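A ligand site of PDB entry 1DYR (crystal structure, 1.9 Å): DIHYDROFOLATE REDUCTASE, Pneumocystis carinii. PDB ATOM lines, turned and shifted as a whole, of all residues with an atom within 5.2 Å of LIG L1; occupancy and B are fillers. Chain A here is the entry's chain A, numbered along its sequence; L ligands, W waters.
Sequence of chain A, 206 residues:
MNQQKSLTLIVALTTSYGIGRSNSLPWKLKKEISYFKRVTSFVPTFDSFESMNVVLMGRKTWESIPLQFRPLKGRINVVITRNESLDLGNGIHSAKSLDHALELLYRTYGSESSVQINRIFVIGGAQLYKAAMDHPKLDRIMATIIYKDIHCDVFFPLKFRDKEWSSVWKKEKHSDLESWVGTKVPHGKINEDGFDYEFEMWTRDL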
ATOM      1  N   ILE A  10      32.041  12.692   7.416  1.00  0.00           N
ATOM      2  CA  ILE A  10      31.882  13.091   6.024  1.00  0.00           C
ATOM      3  C   ILE A  10      31.018  14.339   5.919  1.00  0.00           C
ATOM      4  O   ILE A  10      29.954  14.375   6.527  1.00  0.00           O
ATOM      5  CB  ILE A  10      31.372  11.843   5.199  1.00  0.00           C
ATOM      6  CG1 ILE A  10      31.259  12.281   3.699  1.00  0.00           C
ATOM      7  CG2 ILE A  10      30.000  11.327   5.748  1.00  0.00           C
ATOM      8  CD1 ILE A  10      31.460  11.172   2.664  1.00  0.00           C
ATOM      9  N   VAL A  11      31.524  15.332   5.144  1.00  0.00           N
ATOM     10  CA  VAL A  11      30.926  16.675   5.078  1.00  0.00           C
ATOM     11  C   VAL A  11      31.198  17.328   3.742  1.00  0.00           C
ATOM     12  O   VAL A  11      32.226  16.975   3.152  1.00  0.00           O
ATOM     13  CB  VAL A  11      31.520  17.550   6.241  1.00  0.00           C
ATOM     14  CG1 VAL A  11      33.002  17.606   6.192  1.00  0.00           C
ATOM     15  CG2 VAL A  11      30.859  18.897   6.349  1.00  0.00           C
ATOM     16  N   ALA A  12      30.301  18.156   3.288  1.00  0.00           N
ATOM     17  CA  ALA A  12      30.474  19.010   2.097  1.00  0.00           C
ATOM     18  C   ALA A  12      30.377  20.454   2.609  1.00  0.00           C
ATOM     19  O   ALA A  12      29.389  20.724   3.290  1.00  0.00           O
ATOM     20  CB  ALA A  12      29.428  18.790   0.972  1.00  0.00           C
ATOM     21  N   LEU A  13      31.395  21.259   2.350  1.00  0.00           N
ATOM     22  CA  LEU A  13      31.485  22.586   2.949  1.00  0.00           C
ATOM     23  C   LEU A  13      32.045  23.618   1.985  1.00  0.00           C
ATOM     24  O   LEU A  13      32.817  23.263   1.116  1.00  0.00           O
ATOM     25  CB  LEU A  13      32.282  22.453   4.269  1.00  0.00           C
ATOM     26  CG  LEU A  13      33.771  22.239   4.350  1.00  0.00           C
ATOM     27  CD1 LEU A  13      34.153  22.453   5.844  1.00  0.00           C
ATOM     28  CD2 LEU A  13      34.224  20.866   3.972  1.00  0.00           C
ATOM     29  N   ILE A  19      27.741  24.969   5.893  1.00  0.00           N
ATOM     30  CA  ILE A  19      27.244  23.602   5.653  1.00  0.00           C
ATOM     31  C   ILE A  19      25.754  23.536   5.370  1.00  0.00           C
ATOM     32  O   ILE A  19      25.389  22.447   4.908  1.00  0.00           O
ATOM     33  CB  ILE A  19      27.682  22.477   6.648  1.00  0.00           C
ATOM     34  CG1 ILE A  19      27.228  22.872   8.108  1.00  0.00           C
ATOM     35  CG2 ILE A  19      29.199  22.199   6.601  1.00  0.00           C
ATOM     36  CD1 ILE A  19      27.310  21.649   9.093  1.00  0.00           C
ATOM     37  N   GLY A  20      24.959  24.577   5.652  1.00  0.00           N
ATOM     38  CA  GLY A  20      23.565  24.447   5.221  1.00  0.00           C
ATOM     39  C   GLY A  20      22.851  25.784   5.377  1.00  0.00           C
ATOM     40  O   GLY A  20      23.508  26.721   5.766  1.00  0.00           O
ATOM     41  N   ARG A  21      21.595  25.820   5.003  1.00  0.00           N
ATOM     42  CA  ARG A  21      20.750  27.031   5.080  1.00  0.00           C
ATOM     43  C   ARG A  21      19.322  26.512   5.119  1.00  0.00           C
ATOM     44  O   ARG A  21      18.982  25.679   4.225  1.00  0.00           O
ATOM     45  CB  ARG A  21      20.939  27.855   3.796  1.00  0.00           C
ATOM     46  CG  ARG A  21      20.003  28.969   3.426  1.00  0.00           C
ATOM     47  CD  ARG A  21      20.537  30.334   3.667  1.00  0.00           C
ATOM     48  NE  ARG A  21      19.650  31.292   4.253  1.00  0.00           N
ATOM     49  CZ  ARG A  21      18.832  32.156   3.663  1.00  0.00           C
ATOM     50  NH1 ARG A  21      18.692  32.265   2.340  1.00  0.00           N
ATOM     51  NH2 ARG A  21      18.106  32.981   4.414  1.00  0.00           N
ATOM     52  N   SER A  22      18.489  26.921   6.030  1.00  0.00           N
ATOM     53  CA  SER A  22      17.036  26.612   5.961  1.00  0.00           C
ATOM     54  C   SER A  22      16.788  25.103   6.049  1.00  0.00           C
ATOM     55  O   SER A  22      15.855  24.540   5.399  1.00  0.00           O
ATOM     56  CB  SER A  22      16.331  27.150   4.726  1.00  0.00           C
ATOM     57  OG  SER A  22      16.689  28.421   4.333  1.00  0.00           O
ATOM     58  N   ASN A  23      17.643  24.456   6.841  1.00  0.00           N
ATOM     59  CA  ASN A  23      17.515  23.011   7.107  1.00  0.00           C
ATOM     60  C   ASN A  23      17.606  22.195   5.828  1.00  0.00           C
ATOM     61  O   ASN A  23      16.925  21.148   5.705  1.00  0.00           O
ATOM     62  CB  ASN A  23      16.225  22.775   7.927  1.00  0.00           C
ATOM     63  CG  ASN A  23      16.424  23.193   9.380  1.00  0.00           C
ATOM     64  OD1 ASN A  23      17.245  22.576  10.076  1.00  0.00           O
ATOM     65  ND2 ASN A  23      15.709  24.234   9.802  1.00  0.00           N
ATOM     66  N   SER A  24      18.397  22.673   4.898  1.00  0.00           N
ATOM     67  CA  SER A  24      18.694  22.000   3.623  1.00  0.00           C
ATOM     68  C   SER A  24      20.116  22.338   3.202  1.00  0.00           C
ATOM     69  O   SER A  24      20.758  23.236   3.765  1.00  0.00           O
ATOM     70  CB  SER A  24      17.779  22.516   2.495  1.00  0.00           C
ATOM     71  OG  SER A  24      16.475  22.767   2.950  1.00  0.00           O
ATOM     72  N   LEU A  25      20.571  21.664   2.177  1.00  0.00           N
ATOM     73  CA  LEU A  25      21.784  22.074   1.422  1.00  0.00           C
ATOM     74  C   LEU A  25      21.446  23.217   0.483  1.00  0.00           C
ATOM     75  O   LEU A  25      20.452  23.178  -0.286  1.00  0.00           O
ATOM     76  CB  LEU A  25      22.247  20.780   0.759  1.00  0.00           C
ATOM     77  CG  LEU A  25      23.302  19.869   1.288  1.00  0.00           C
ATOM     78  CD1 LEU A  25      23.595  19.890   2.751  1.00  0.00           C
ATOM     79  CD2 LEU A  25      22.937  18.443   0.820  1.00  0.00           C
ATOM     80  N   TRP A  27      22.864  23.683  -2.141  1.00  0.00           N
ATOM     81  CA  TRP A  27      23.320  23.309  -3.520  1.00  0.00           C
ATOM     82  C   TRP A  27      22.698  21.995  -3.951  1.00  0.00           C
ATOM     83  O   TRP A  27      22.420  21.161  -3.068  1.00  0.00           O
ATOM     84  CB  TRP A  27      24.851  23.241  -3.549  1.00  0.00           C
ATOM     85  CG  TRP A  27      25.448  22.463  -2.419  1.00  0.00           C
ATOM     86  CD1 TRP A  27      25.527  21.129  -2.291  1.00  0.00           C
ATOM     87  CD2 TRP A  27      26.037  23.041  -1.232  1.00  0.00           C
ATOM     88  NE1 TRP A  27      26.151  20.814  -1.081  1.00  0.00           N
ATOM     89  CE2 TRP A  27      26.461  21.960  -0.423  1.00  0.00           C
ATOM     90  CE3 TRP A  27      26.236  24.347  -0.790  1.00  0.00           C
ATOM     91  CZ2 TRP A  27      27.097  22.142   0.802  1.00  0.00           C
ATOM     92  CZ3 TRP A  27      26.864  24.529   0.446  1.00  0.00           C
ATOM     93  CH2 TRP A  27      27.288  23.435   1.211  1.00  0.00           C
ATOM     94  N   GLY A  58      22.252  13.348  13.374  1.00  0.00           N
ATOM     95  CA  GLY A  58      21.391  14.157  14.208  1.00  0.00           C
ATOM     96  C   GLY A  58      19.954  14.071  13.665  1.00  0.00           C
ATOM     97  O   GLY A  58      19.662  13.741  12.495  1.00  0.00           O
ATOM     98  N   ARG A  59      19.023  14.344  14.574  1.00  0.00           N
ATOM     99  CA  ARG A  59      17.591  14.214  14.299  1.00  0.00           C
ATOM    100  C   ARG A  59      17.149  15.158  13.204  1.00  0.00           C
ATOM    101  O   ARG A  59      16.297  14.788  12.384  1.00  0.00           O
ATOM    102  CB  ARG A  59      16.790  14.583  15.570  1.00  0.00           C
ATOM    103  CG  ARG A  59      15.345  14.227  15.463  1.00  0.00           C
ATOM    104  CD  ARG A  59      14.390  15.276  15.715  1.00  0.00           C
ATOM    105  NE  ARG A  59      14.711  16.206  16.779  1.00  0.00           N
ATOM    106  CZ  ARG A  59      14.352  17.498  16.769  1.00  0.00           C
ATOM    107  NH1 ARG A  59      13.637  18.013  15.764  1.00  0.00           N
ATOM    108  NH2 ARG A  59      14.762  18.310  17.733  1.00  0.00           N
ATOM    109  N   LYS A  60      17.642  16.382  13.240  1.00  0.00           N
ATOM    110  CA  LYS A  60      17.256  17.376  12.187  1.00  0.00           C
ATOM    111  C   LYS A  60      17.801  17.018  10.822  1.00  0.00           C
ATOM    112  O   LYS A  60      17.174  17.366   9.777  1.00  0.00           O
ATOM    113  CB  LYS A  60      17.564  18.782  12.542  1.00  0.00           C
ATOM    114  CG  LYS A  60      16.841  19.377  13.737  1.00  0.00           C
ATOM    115  CD  LYS A  60      17.340  20.739  14.183  1.00  0.00           C
ATOM    116  CE  LYS A  60      17.134  21.838  13.131  1.00  0.00           C
ATOM    117  NZ  LYS A  60      17.248  23.188  13.730  1.00  0.00           N
ATOM    118  N   THR A  61      18.949  16.402  10.747  1.00  0.00           N
ATOM    119  CA  THR A  61      19.434  15.834   9.462  1.00  0.00           C
ATOM    120  C   THR A  61      18.509  14.722   9.023  1.00  0.00           C
ATOM    121  O   THR A  61      18.116  14.705   7.821  1.00  0.00           O
ATOM    122  CB  THR A  61      20.934  15.350   9.562  1.00  0.00           C
ATOM    123  OG1 THR A  61      21.667  16.593   9.855  1.00  0.00           O
ATOM    124  CG2 THR A  61      21.481  14.702   8.287  1.00  0.00           C
ATOM    125  N   SER A  64      15.718  16.131   7.513  1.00  0.00           N
ATOM    126  CA  SER A  64      16.029  16.831   6.258  1.00  0.00           C
ATOM    127  C   SER A  64      16.095  15.932   5.050  1.00  0.00           C
ATOM    128  O   SER A  64      15.920  16.464   3.937  1.00  0.00           O
ATOM    129  CB  SER A  64      17.280  17.691   6.377  1.00  0.00           C
ATOM    130  OG  SER A  64      16.979  18.674   7.400  1.00  0.00           O
ATOM    131  N   ILE A  80      20.594  10.208  16.441  1.00  0.00           N
ATOM    132  CA  ILE A  80      20.986  10.648  17.809  1.00  0.00           C
ATOM    133  C   ILE A  80      19.936  11.674  18.192  1.00  0.00           C
ATOM    134  O   ILE A  80      19.577  12.598  17.398  1.00  0.00           O
ATOM    135  CB  ILE A  80      22.456  11.207  17.774  1.00  0.00           C
ATOM    136  CG1 ILE A  80      23.460  10.287  17.091  1.00  0.00           C
ATOM    137  CG2 ILE A  80      22.936  11.687  19.190  1.00  0.00           C
ATOM    138  CD1 ILE A  80      23.700   8.907  17.684  1.00  0.00           C
ATOM    139  N   THR A  81      19.332  11.476  19.358  1.00  0.00           N
ATOM    140  CA  THR A  81      18.181  12.316  19.800  1.00  0.00           C
ATOM    141  C   THR A  81      18.040  12.085  21.302  1.00  0.00           C
ATOM    142  O   THR A  81      18.171  10.888  21.671  1.00  0.00           O
ATOM    143  CB  THR A  81      16.837  11.931  19.044  1.00  0.00           C
ATOM    144  OG1 THR A  81      15.774  12.738  19.632  1.00  0.00           O
ATOM    145  CG2 THR A  81      16.423  10.453  19.034  1.00  0.00           C
ATOM    146  N   ARG A  82      17.851  13.091  22.100  1.00  0.00           N
ATOM    147  CA  ARG A  82      17.466  12.841  23.526  1.00  0.00           C
ATOM    148  C   ARG A  82      15.952  12.599  23.614  1.00  0.00           C
ATOM    149  O   ARG A  82      15.408  11.843  24.421  1.00  0.00           O
ATOM    150  CB  ARG A  82      17.725  14.045  24.411  1.00  0.00           C
ATOM    151  CG  ARG A  82      19.204  14.281  24.685  1.00  0.00           C
ATOM    152  CD  ARG A  82      19.445  15.719  24.407  1.00  0.00           C
ATOM    153  NE  ARG A  82      20.759  16.209  24.769  1.00  0.00           N
ATOM    154  CZ  ARG A  82      21.179  17.400  24.317  1.00  0.00           C
ATOM    155  NH1 ARG A  82      20.418  18.256  23.611  1.00  0.00           N
ATOM    156  NH2 ARG A  82      22.467  17.710  24.501  1.00  0.00           N
ATOM    157  N   ASN A  83      15.301  13.308  22.744  1.00  0.00           N
ATOM    158  CA  ASN A  83      13.837  13.372  22.629  1.00  0.00           C
ATOM    159  C   ASN A  83      13.385  12.193  21.786  1.00  0.00           C
ATOM    160  O   ASN A  83      12.483  12.297  20.926  1.00  0.00           O
ATOM    161  CB  ASN A  83      13.458  14.757  22.101  1.00  0.00           C
ATOM    162  CG  ASN A  83      13.014  15.701  23.185  1.00  0.00           C
ATOM    163  OD1 ASN A  83      12.814  15.283  24.335  1.00  0.00           O
ATOM    164  ND2 ASN A  83      12.830  16.968  22.803  1.00  0.00           N
ATOM    165  N   LYS A  96      20.968   8.192  22.549  1.00  0.00           N
ATOM    166  CA  LYS A  96      20.851   9.493  23.231  1.00  0.00           C
ATOM    167  C   LYS A  96      22.112  10.287  23.119  1.00  0.00           C
ATOM    168  O   LYS A  96      22.140  11.500  23.451  1.00  0.00           O
ATOM    169  CB  LYS A  96      20.193   9.445  24.576  1.00  0.00           C
ATOM    170  CG  LYS A  96      20.991   9.096  25.818  1.00  0.00           C
ATOM    171  CD  LYS A  96      20.041   8.746  27.000  1.00  0.00           C
ATOM    172  CE  LYS A  96      20.755   7.961  28.076  1.00  0.00           C
ATOM    173  NZ  LYS A  96      19.794   7.260  28.977  1.00  0.00           N
ATOM    174  N   SER A  97      23.165   9.680  22.664  1.00  0.00           N
ATOM    175  CA  SER A  97      24.453  10.377  22.441  1.00  0.00           C
ATOM    176  C   SER A  97      25.313   9.548  21.525  1.00  0.00           C
ATOM    177  O   SER A  97      24.998   8.412  21.181  1.00  0.00           O
ATOM    178  CB  SER A  97      25.103  10.725  23.781  1.00  0.00           C
ATOM    179  OG  SER A  97      25.881   9.649  24.262  1.00  0.00           O
ATOM    180  N   ILE A 123      27.469  11.636   9.680  1.00  0.00           N
ATOM    181  CA  ILE A 123      27.103  12.346   8.450  1.00  0.00           C
ATOM    182  C   ILE A 123      26.424  13.660   8.668  1.00  0.00           C
ATOM    183  O   ILE A 123      25.861  14.275   7.732  1.00  0.00           O
ATOM    184  CB  ILE A 123      26.344  11.355   7.526  1.00  0.00           C
ATOM    185  CG1 ILE A 123      24.918  11.167   8.130  1.00  0.00           C
ATOM    186  CG2 ILE A 123      27.022   9.982   7.308  1.00  0.00           C
ATOM    187  CD1 ILE A 123      23.724  11.052   7.140  1.00  0.00           C
ATOM    188  N   GLY A 124      26.375  14.149   9.944  1.00  0.00           N
ATOM    189  CA  GLY A 124      25.881  15.498  10.204  1.00  0.00           C
ATOM    190  C   GLY A 124      24.771  15.549  11.236  1.00  0.00           C
ATOM    191  O   GLY A 124      24.407  14.475  11.738  1.00  0.00           O
ATOM    192  N   GLY A 125      24.268  16.705  11.605  1.00  0.00           N
ATOM    193  CA  GLY A 125      24.550  18.053  11.199  1.00  0.00           C
ATOM    194  C   GLY A 125      25.568  18.706  12.089  1.00  0.00           C
ATOM    195  O   GLY A 125      26.450  18.019  12.646  1.00  0.00           O
ATOM    196  N   ALA A 126      25.483  20.000  12.195  1.00  0.00           N
ATOM    197  CA  ALA A 126      26.516  20.796  12.883  1.00  0.00           C
ATOM    198  C   ALA A 126      26.657  20.380  14.342  1.00  0.00           C
ATOM    199  O   ALA A 126      27.734  20.162  14.900  1.00  0.00           O
ATOM    200  CB  ALA A 126      26.104  22.271  12.753  1.00  0.00           C
ATOM    201  N   GLN A 127      25.521  20.284  15.038  1.00  0.00           N
ATOM    202  CA  GLN A 127      25.515  19.799  16.457  1.00  0.00           C
ATOM    203  C   GLN A 127      26.230  18.493  16.655  1.00  0.00           C
ATOM    204  O   GLN A 127      27.105  18.309  17.539  1.00  0.00           O
ATOM    205  CB  GLN A 127      24.060  19.731  16.924  1.00  0.00           C
ATOM    206  CG  GLN A 127      23.967  19.964  18.442  1.00  0.00           C
ATOM    207  CD  GLN A 127      22.497  20.095  18.800  1.00  0.00           C
ATOM    208  OE1 GLN A 127      21.984  19.329  19.612  1.00  0.00           O
ATOM    209  NE2 GLN A 127      21.831  21.028  18.138  1.00  0.00           N
ATOM    210  N   LEU A 128      25.878  17.437  15.911  1.00  0.00           N
ATOM    211  CA  LEU A 128      26.595  16.150  15.977  1.00  0.00           C
ATOM    212  C   LEU A 128      28.047  16.268  15.562  1.00  0.00           C
ATOM    213  O   LEU A 128      28.929  15.508  16.075  1.00  0.00           O
ATOM    214  CB  LEU A 128      25.868  15.079  15.211  1.00  0.00           C
ATOM    215  CG  LEU A 128      25.789  13.640  15.556  1.00  0.00           C
ATOM    216  CD1 LEU A 128      26.080  12.723  14.410  1.00  0.00           C
ATOM    217  CD2 LEU A 128      26.428  13.122  16.822  1.00  0.00           C
ATOM    218  N   TYR A 129      28.331  17.092  14.577  1.00  0.00           N
ATOM    219  CA  TYR A 129      29.737  17.284  14.161  1.00  0.00           C
ATOM    220  C   TYR A 129      30.554  17.828  15.343  1.00  0.00           C
ATOM    221  O   TYR A 129      31.724  17.496  15.390  1.00  0.00           O
ATOM    222  CB  TYR A 129      29.870  18.268  12.976  1.00  0.00           C
ATOM    223  CG  TYR A 129      29.488  17.728  11.607  1.00  0.00           C
ATOM    224  CD1 TYR A 129      29.793  16.403  11.207  1.00  0.00           C
ATOM    225  CD2 TYR A 129      28.881  18.574  10.707  1.00  0.00           C
ATOM    226  CE1 TYR A 129      29.431  15.950   9.933  1.00  0.00           C
ATOM    227  CE2 TYR A 129      28.575  18.140   9.405  1.00  0.00           C
ATOM    228  CZ  TYR A 129      28.873  16.861   9.043  1.00  0.00           C
ATOM    229  OH  TYR A 129      28.533  16.411   7.758  1.00  0.00           O
ATOM    230  N   ALA A 131      30.048  17.372  18.666  1.00  0.00           N
ATOM    231  CA  ALA A 131      30.344  16.169  19.450  1.00  0.00           C
ATOM    232  C   ALA A 131      31.369  15.249  18.844  1.00  0.00           C
ATOM    233  O   ALA A 131      32.284  14.749  19.574  1.00  0.00           O
ATOM    234  CB  ALA A 131      29.018  15.432  19.699  1.00  0.00           C
ATOM    235  N   VAL A 154      24.427  27.858   8.954  1.00  0.00           N
ATOM    236  CA  VAL A 154      24.968  26.769   9.779  1.00  0.00           C
ATOM    237  C   VAL A 154      26.400  26.491   9.279  1.00  0.00           C
ATOM    238  O   VAL A 154      26.599  26.362   8.051  1.00  0.00           O
ATOM    239  CB  VAL A 154      24.123  25.460   9.595  1.00  0.00           C
ATOM    240  CG1 VAL A 154      24.588  24.359  10.549  1.00  0.00           C
ATOM    241  CG2 VAL A 154      22.653  25.668   9.767  1.00  0.00           C
HETATM  242  P1  LIG L   1      21.589  17.969  13.665  1.00  0.00           P
HETATM  243  O1  LIG L   1      22.887  17.666  14.249  1.00  0.00           O
HETATM  244  O2  LIG L   1      21.367  17.162  12.418  1.00  0.00           O
HETATM  245  O3  LIG L   1      20.407  17.597  14.664  1.00  0.00           O
HETATM  246  C1  LIG L   1      20.377  18.282  15.945  1.00  0.00           C
HETATM  247  C2  LIG L   1      19.614  17.397  16.915  1.00  0.00           C
HETATM  248  O4  LIG L   1      20.229  16.098  17.002  1.00  0.00           O
HETATM  249  C3  LIG L   1      19.534  17.940  18.371  1.00  0.00           C
HETATM  250  O5  LIG L   1      18.559  18.995  18.369  1.00  0.00           O
HETATM  251  C4  LIG L   1      19.291  16.592  19.114  1.00  0.00           C
HETATM  252  O6  LIG L   1      18.022  15.892  18.938  1.00  0.00           O
HETATM  253  C5  LIG L   1      20.298  15.759  18.336  1.00  0.00           C
HETATM  254  N1  LIG L   1      21.659  15.806  18.708  1.00  0.00           N
HETATM  255  C6  LIG L   1      22.731  16.269  17.927  1.00  0.00           C
HETATM  256  N2  LIG L   1      23.885  16.187  18.551  1.00  0.00           N
HETATM  257  C7  LIG L   1      23.558  15.608  19.758  1.00  0.00           C
HETATM  258  C8  LIG L   1      24.373  15.172  20.819  1.00  0.00           C
HETATM  259  N3  LIG L   1      25.699  15.321  20.785  1.00  0.00           N
HETATM  260  N4  LIG L   1      23.745  14.656  21.880  1.00  0.00           N
HETATM  261  C9  LIG L   1      22.394  14.510  21.860  1.00  0.00           C
HETATM  262  N5  LIG L   1      21.560  14.820  20.926  1.00  0.00           N
HETATM  263  C10 LIG L   1      22.219  15.385  19.870  1.00  0.00           C
HETATM  264  O7  LIG L   1      21.319  19.450  13.420  1.00  0.00           O
HETATM  265  P2  LIG L   1      21.854  20.910  13.062  1.00  0.00           P
HETATM  266  O8  LIG L   1      22.978  21.296  13.900  1.00  0.00           O
HETATM  267  O9  LIG L   1      20.731  21.833  13.251  1.00  0.00           O
HETATM  268  O10 LIG L   1      22.303  20.779  11.536  1.00  0.00           O
HETATM  269  C11 LIG L   1      21.286  20.733  10.511  1.00  0.00           C
HETATM  270  C12 LIG L   1      21.805  21.405   9.280  1.00  0.00           C
HETATM  271  O11 LIG L   1      23.045  20.741   8.842  1.00  0.00           O
HETATM  272  C13 LIG L   1      20.863  21.428   8.072  1.00  0.00           C
HETATM  273  O12 LIG L   1      20.943  22.740   7.437  1.00  0.00           O
HETATM  274  C14 LIG L   1      21.462  20.327   7.202  1.00  0.00           C
HETATM  275  O13 LIG L   1      21.100  20.507   5.809  1.00  0.00           O
HETATM  276  C15 LIG L   1      22.931  20.543   7.407  1.00  0.00           C
HETATM  277  N6  LIG L   1      23.783  19.405   7.008  1.00  0.00           N
HETATM  278  C16 LIG L   1      24.810  19.611   6.115  1.00  0.00           C
HETATM  279  C17 LIG L   1      25.624  18.590   5.749  1.00  0.00           C
HETATM  280  C18 LIG L   1      26.791  18.852   4.721  1.00  0.00           C
HETATM  281  O14 LIG L   1      27.522  17.912   4.478  1.00  0.00           O
HETATM  282  N7  LIG L   1      26.851  20.095   4.230  1.00  0.00           N
HETATM  283  C19 LIG L   1      25.510  17.295   6.245  1.00  0.00           C
HETATM  284  C20 LIG L   1      24.428  17.192   7.149  1.00  0.00           C
HETATM  285  C21 LIG L   1      23.585  18.127   7.573  1.00  0.00           C
HETATM  286  P3  LIG L   1      16.676  16.247  19.846  1.00  0.00           P
HETATM  287  O15 LIG L   1      16.639  17.780  19.783  1.00  0.00           O
HETATM  288  O16 LIG L   1      15.571  15.542  19.218  1.00  0.00           O
HETATM  289  O17 LIG L   1      17.020  15.737  21.191  1.00  0.00           O
HETATM  290  C1  LG2 L   2      26.146  14.758   1.904  1.00  0.00           C
HETATM  291  N1  LG2 L   2      27.300  14.858   1.239  1.00  0.00           N
HETATM  292  C2  LG2 L   2      28.388  14.770   1.947  1.00  0.00           C
HETATM  293  N2  LG2 L   2      29.599  14.830   1.324  1.00  0.00           N
HETATM  294  N3  LG2 L   2      28.516  14.558   3.279  1.00  0.00           N
HETATM  295  C3  LG2 L   2      27.349  14.428   3.926  1.00  0.00           C
HETATM  296  N4  LG2 L   2      27.355  14.177   5.256  1.00  0.00           N
HETATM  297  C4  LG2 L   2      26.147  14.490   3.248  1.00  0.00           C
HETATM  298  C5  LG2 L   2      24.826  14.342   4.018  1.00  0.00           C
HETATM  299  C6  LG2 L   2      23.504  14.507   3.260  1.00  0.00           C
HETATM  300  C7  LG2 L   2      22.726  15.609   3.590  1.00  0.00           C
HETATM  301  C8  LG2 L   2      21.485  15.814   2.961  1.00  0.00           C
HETATM  302  O1  LG2 L   2      20.714  16.912   3.227  1.00  0.00           O
HETATM  303  C9  LG2 L   2      20.986  17.629   4.406  1.00  0.00           C
HETATM  304  C10 LG2 L   2      21.061  14.878   1.996  1.00  0.00           C
HETATM  305  O2  LG2 L   2      19.826  15.034   1.346  1.00  0.00           O
HETATM  306  C11 LG2 L   2      20.046  14.774  -0.006  1.00  0.00           C
HETATM  307  C12 LG2 L   2      21.825  13.760   1.691  1.00  0.00           C
HETATM  308  O3  LG2 L   2      21.288  12.902   0.728  1.00  0.00           O
HETATM  309  C13 LG2 L   2      21.965  11.642   0.756  1.00  0.00           C
HETATM  310  C14 LG2 L   2      23.063  13.542   2.317  1.00  0.00           C
HETATM  311  O   HOH W   1      25.704  14.633  24.015  1.00  0.00           O
HETATM  312  O   HOH W   2      12.726  16.076  19.296  1.00  0.00           O
HETATM  313  O   HOH W   3      19.333  20.561  20.890  1.00  0.00           O
HETATM  314  O   HOH W   4      19.953  25.137   8.326  1.00  0.00           O
HETATM  315  O   HOH W   5      27.097  12.899  22.063  1.00  0.00           O
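N of Thr 61 is in hydrogen-bond range of O2 of LIG L1 (3.0 Å). The side-chain hydroxyl of Thr 61 sits at hydrogen-bond distance from an oxygen (O2) of LIG L1. The backbone NH of Arg 59 is in hydrogen-bond range of an oxygen (O4) of LIG L1 (3.2 Å). O16 of LIG L1 is in salt-bridge range of NE of Arg 59 (2.7 Å). N of Ala 12 lies within hydrogen-bond range of O14 of LIG L1, at 3.0 Å. O of Ala 12 lies within hydrogen-bond range of N7 of LIG L1 (2.8 Å). OG1 of Thr 81 sits at hydrogen-bond distance from O16 of LIG L1, at 2.8 Å. A nitrogen (N7) of LIG L1 sits at hydrogen-bond distance from the backbone carbonyl oxygen (O) of Ile 19. The backbone NH (N) of Arg 82 sits at hydrogen-bond distance from an oxygen (O17) of LIG L1 (2.9 Å). An oxygen (O8) of LIG L1 is in hydrogen-bond range of the backbone NH of Gln 127, 3.0 Å away. The backbone NH of Gly 125 is in hydrogen-bond range of an oxygen (O2) of LIG L1, at 3.0 Å. The backbone NH (N) of Ala 126 sits at hydrogen-bond distance from an oxygen (O8) of LIG L1, at 3.3 Å. The backbone carbonyl oxygen (O) of Ser 24 lies close to an oxygen (O13) of LIG L1, at 3.4 Å. The backbone NH (N) of Lys 60 is in hydrogen-bond range of an oxygen (O3) of LIG L1. The side-chain amino group (NZ) of Lys 60 is in salt-bridge range of an oxygen (O9) of LIG L1, at 3.8 Å. O17 of LIG L1 is in hydrogen-bond range of N of Asn 83 (3.4 Å). O1 of LIG L1 sits at hydrogen-bond distance from N of Leu 128, 3.4 Å away. A nitrogen (N4) of LG2 L2 lies within hydrogen-bond range of the backbone carbonyl oxygen (O) of Ile 123 (2.9 Å). O of Ile 10 is in hydrogen-bond range of N4 of LG2 L2, at 2.9 Å.
OG1 of Thr 61 sits at hydrogen-bond distance from N of Gly 125 (3.1 Å). N of Asn 83 lies within hydrogen-bond range of OG1 of Thr 81 (3.2 Å). The backbone NH (N) of Ile 19 is in hydrogen-bond range of the backbone carbonyl oxygen (O) of Val 154 (2.8 Å). The side-chain hydroxyl (OH) of Tyr 129 lies within hydrogen-bond range of the backbone carbonyl oxygen (O) of Ile 123, 3.4 Å away. The side-chain hydroxyl (OG) of Ser 24 sits at hydrogen-bond distance from the backbone carbonyl oxygen (O) of Ser 22 (3.1 Å). The backbone carbonyl oxygen (O) of Asn 23 is in hydrogen-bond range of the side-chain hydroxyl (OG) of Ser 64 (3.0 Å). The side-chain hydroxyl (OH) of Tyr 129 lies within hydrogen-bond range of the backbone carbonyl oxygen (O) of Ile 10. The backbone NH of Gly 58 is in hydrogen-bond range of the backbone carbonyl oxygen of Gly 124 (2.9 Å).
Residues that only touch LIG L1: Val 11, Gly 20, Arg 21, Asn 23, Leu 25, Gly 58, Ile 80, Lys 96, Ile 123, Gly 124, Tyr 129 and Ala 131. Hydrophobic or aromatic side chains within 4 Å of LIG L1: Val 11, Ile 19, Leu 25, Ile 80, Ala 126 and Ala 131. Of the 32 residues printed, 25 come within 4 Å of LIG L1. Along chain A the residues within 4 Å of LIG L1 span positions 11 to 131.
Water W4 lies within hydrogen-bond range of O12 of LIG L1 (2.7 Å), N of Asn 23 (2.8 Å) and N of Ser 22 (3.3 Å). Water W2 bridges an oxygen (O16) of LIG L1 and the guanidinium group of Arg 59. Water W3 bridges O5 of LIG L1 (3.1 Å) and OE1 of Gln 127 (3.2 Å).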
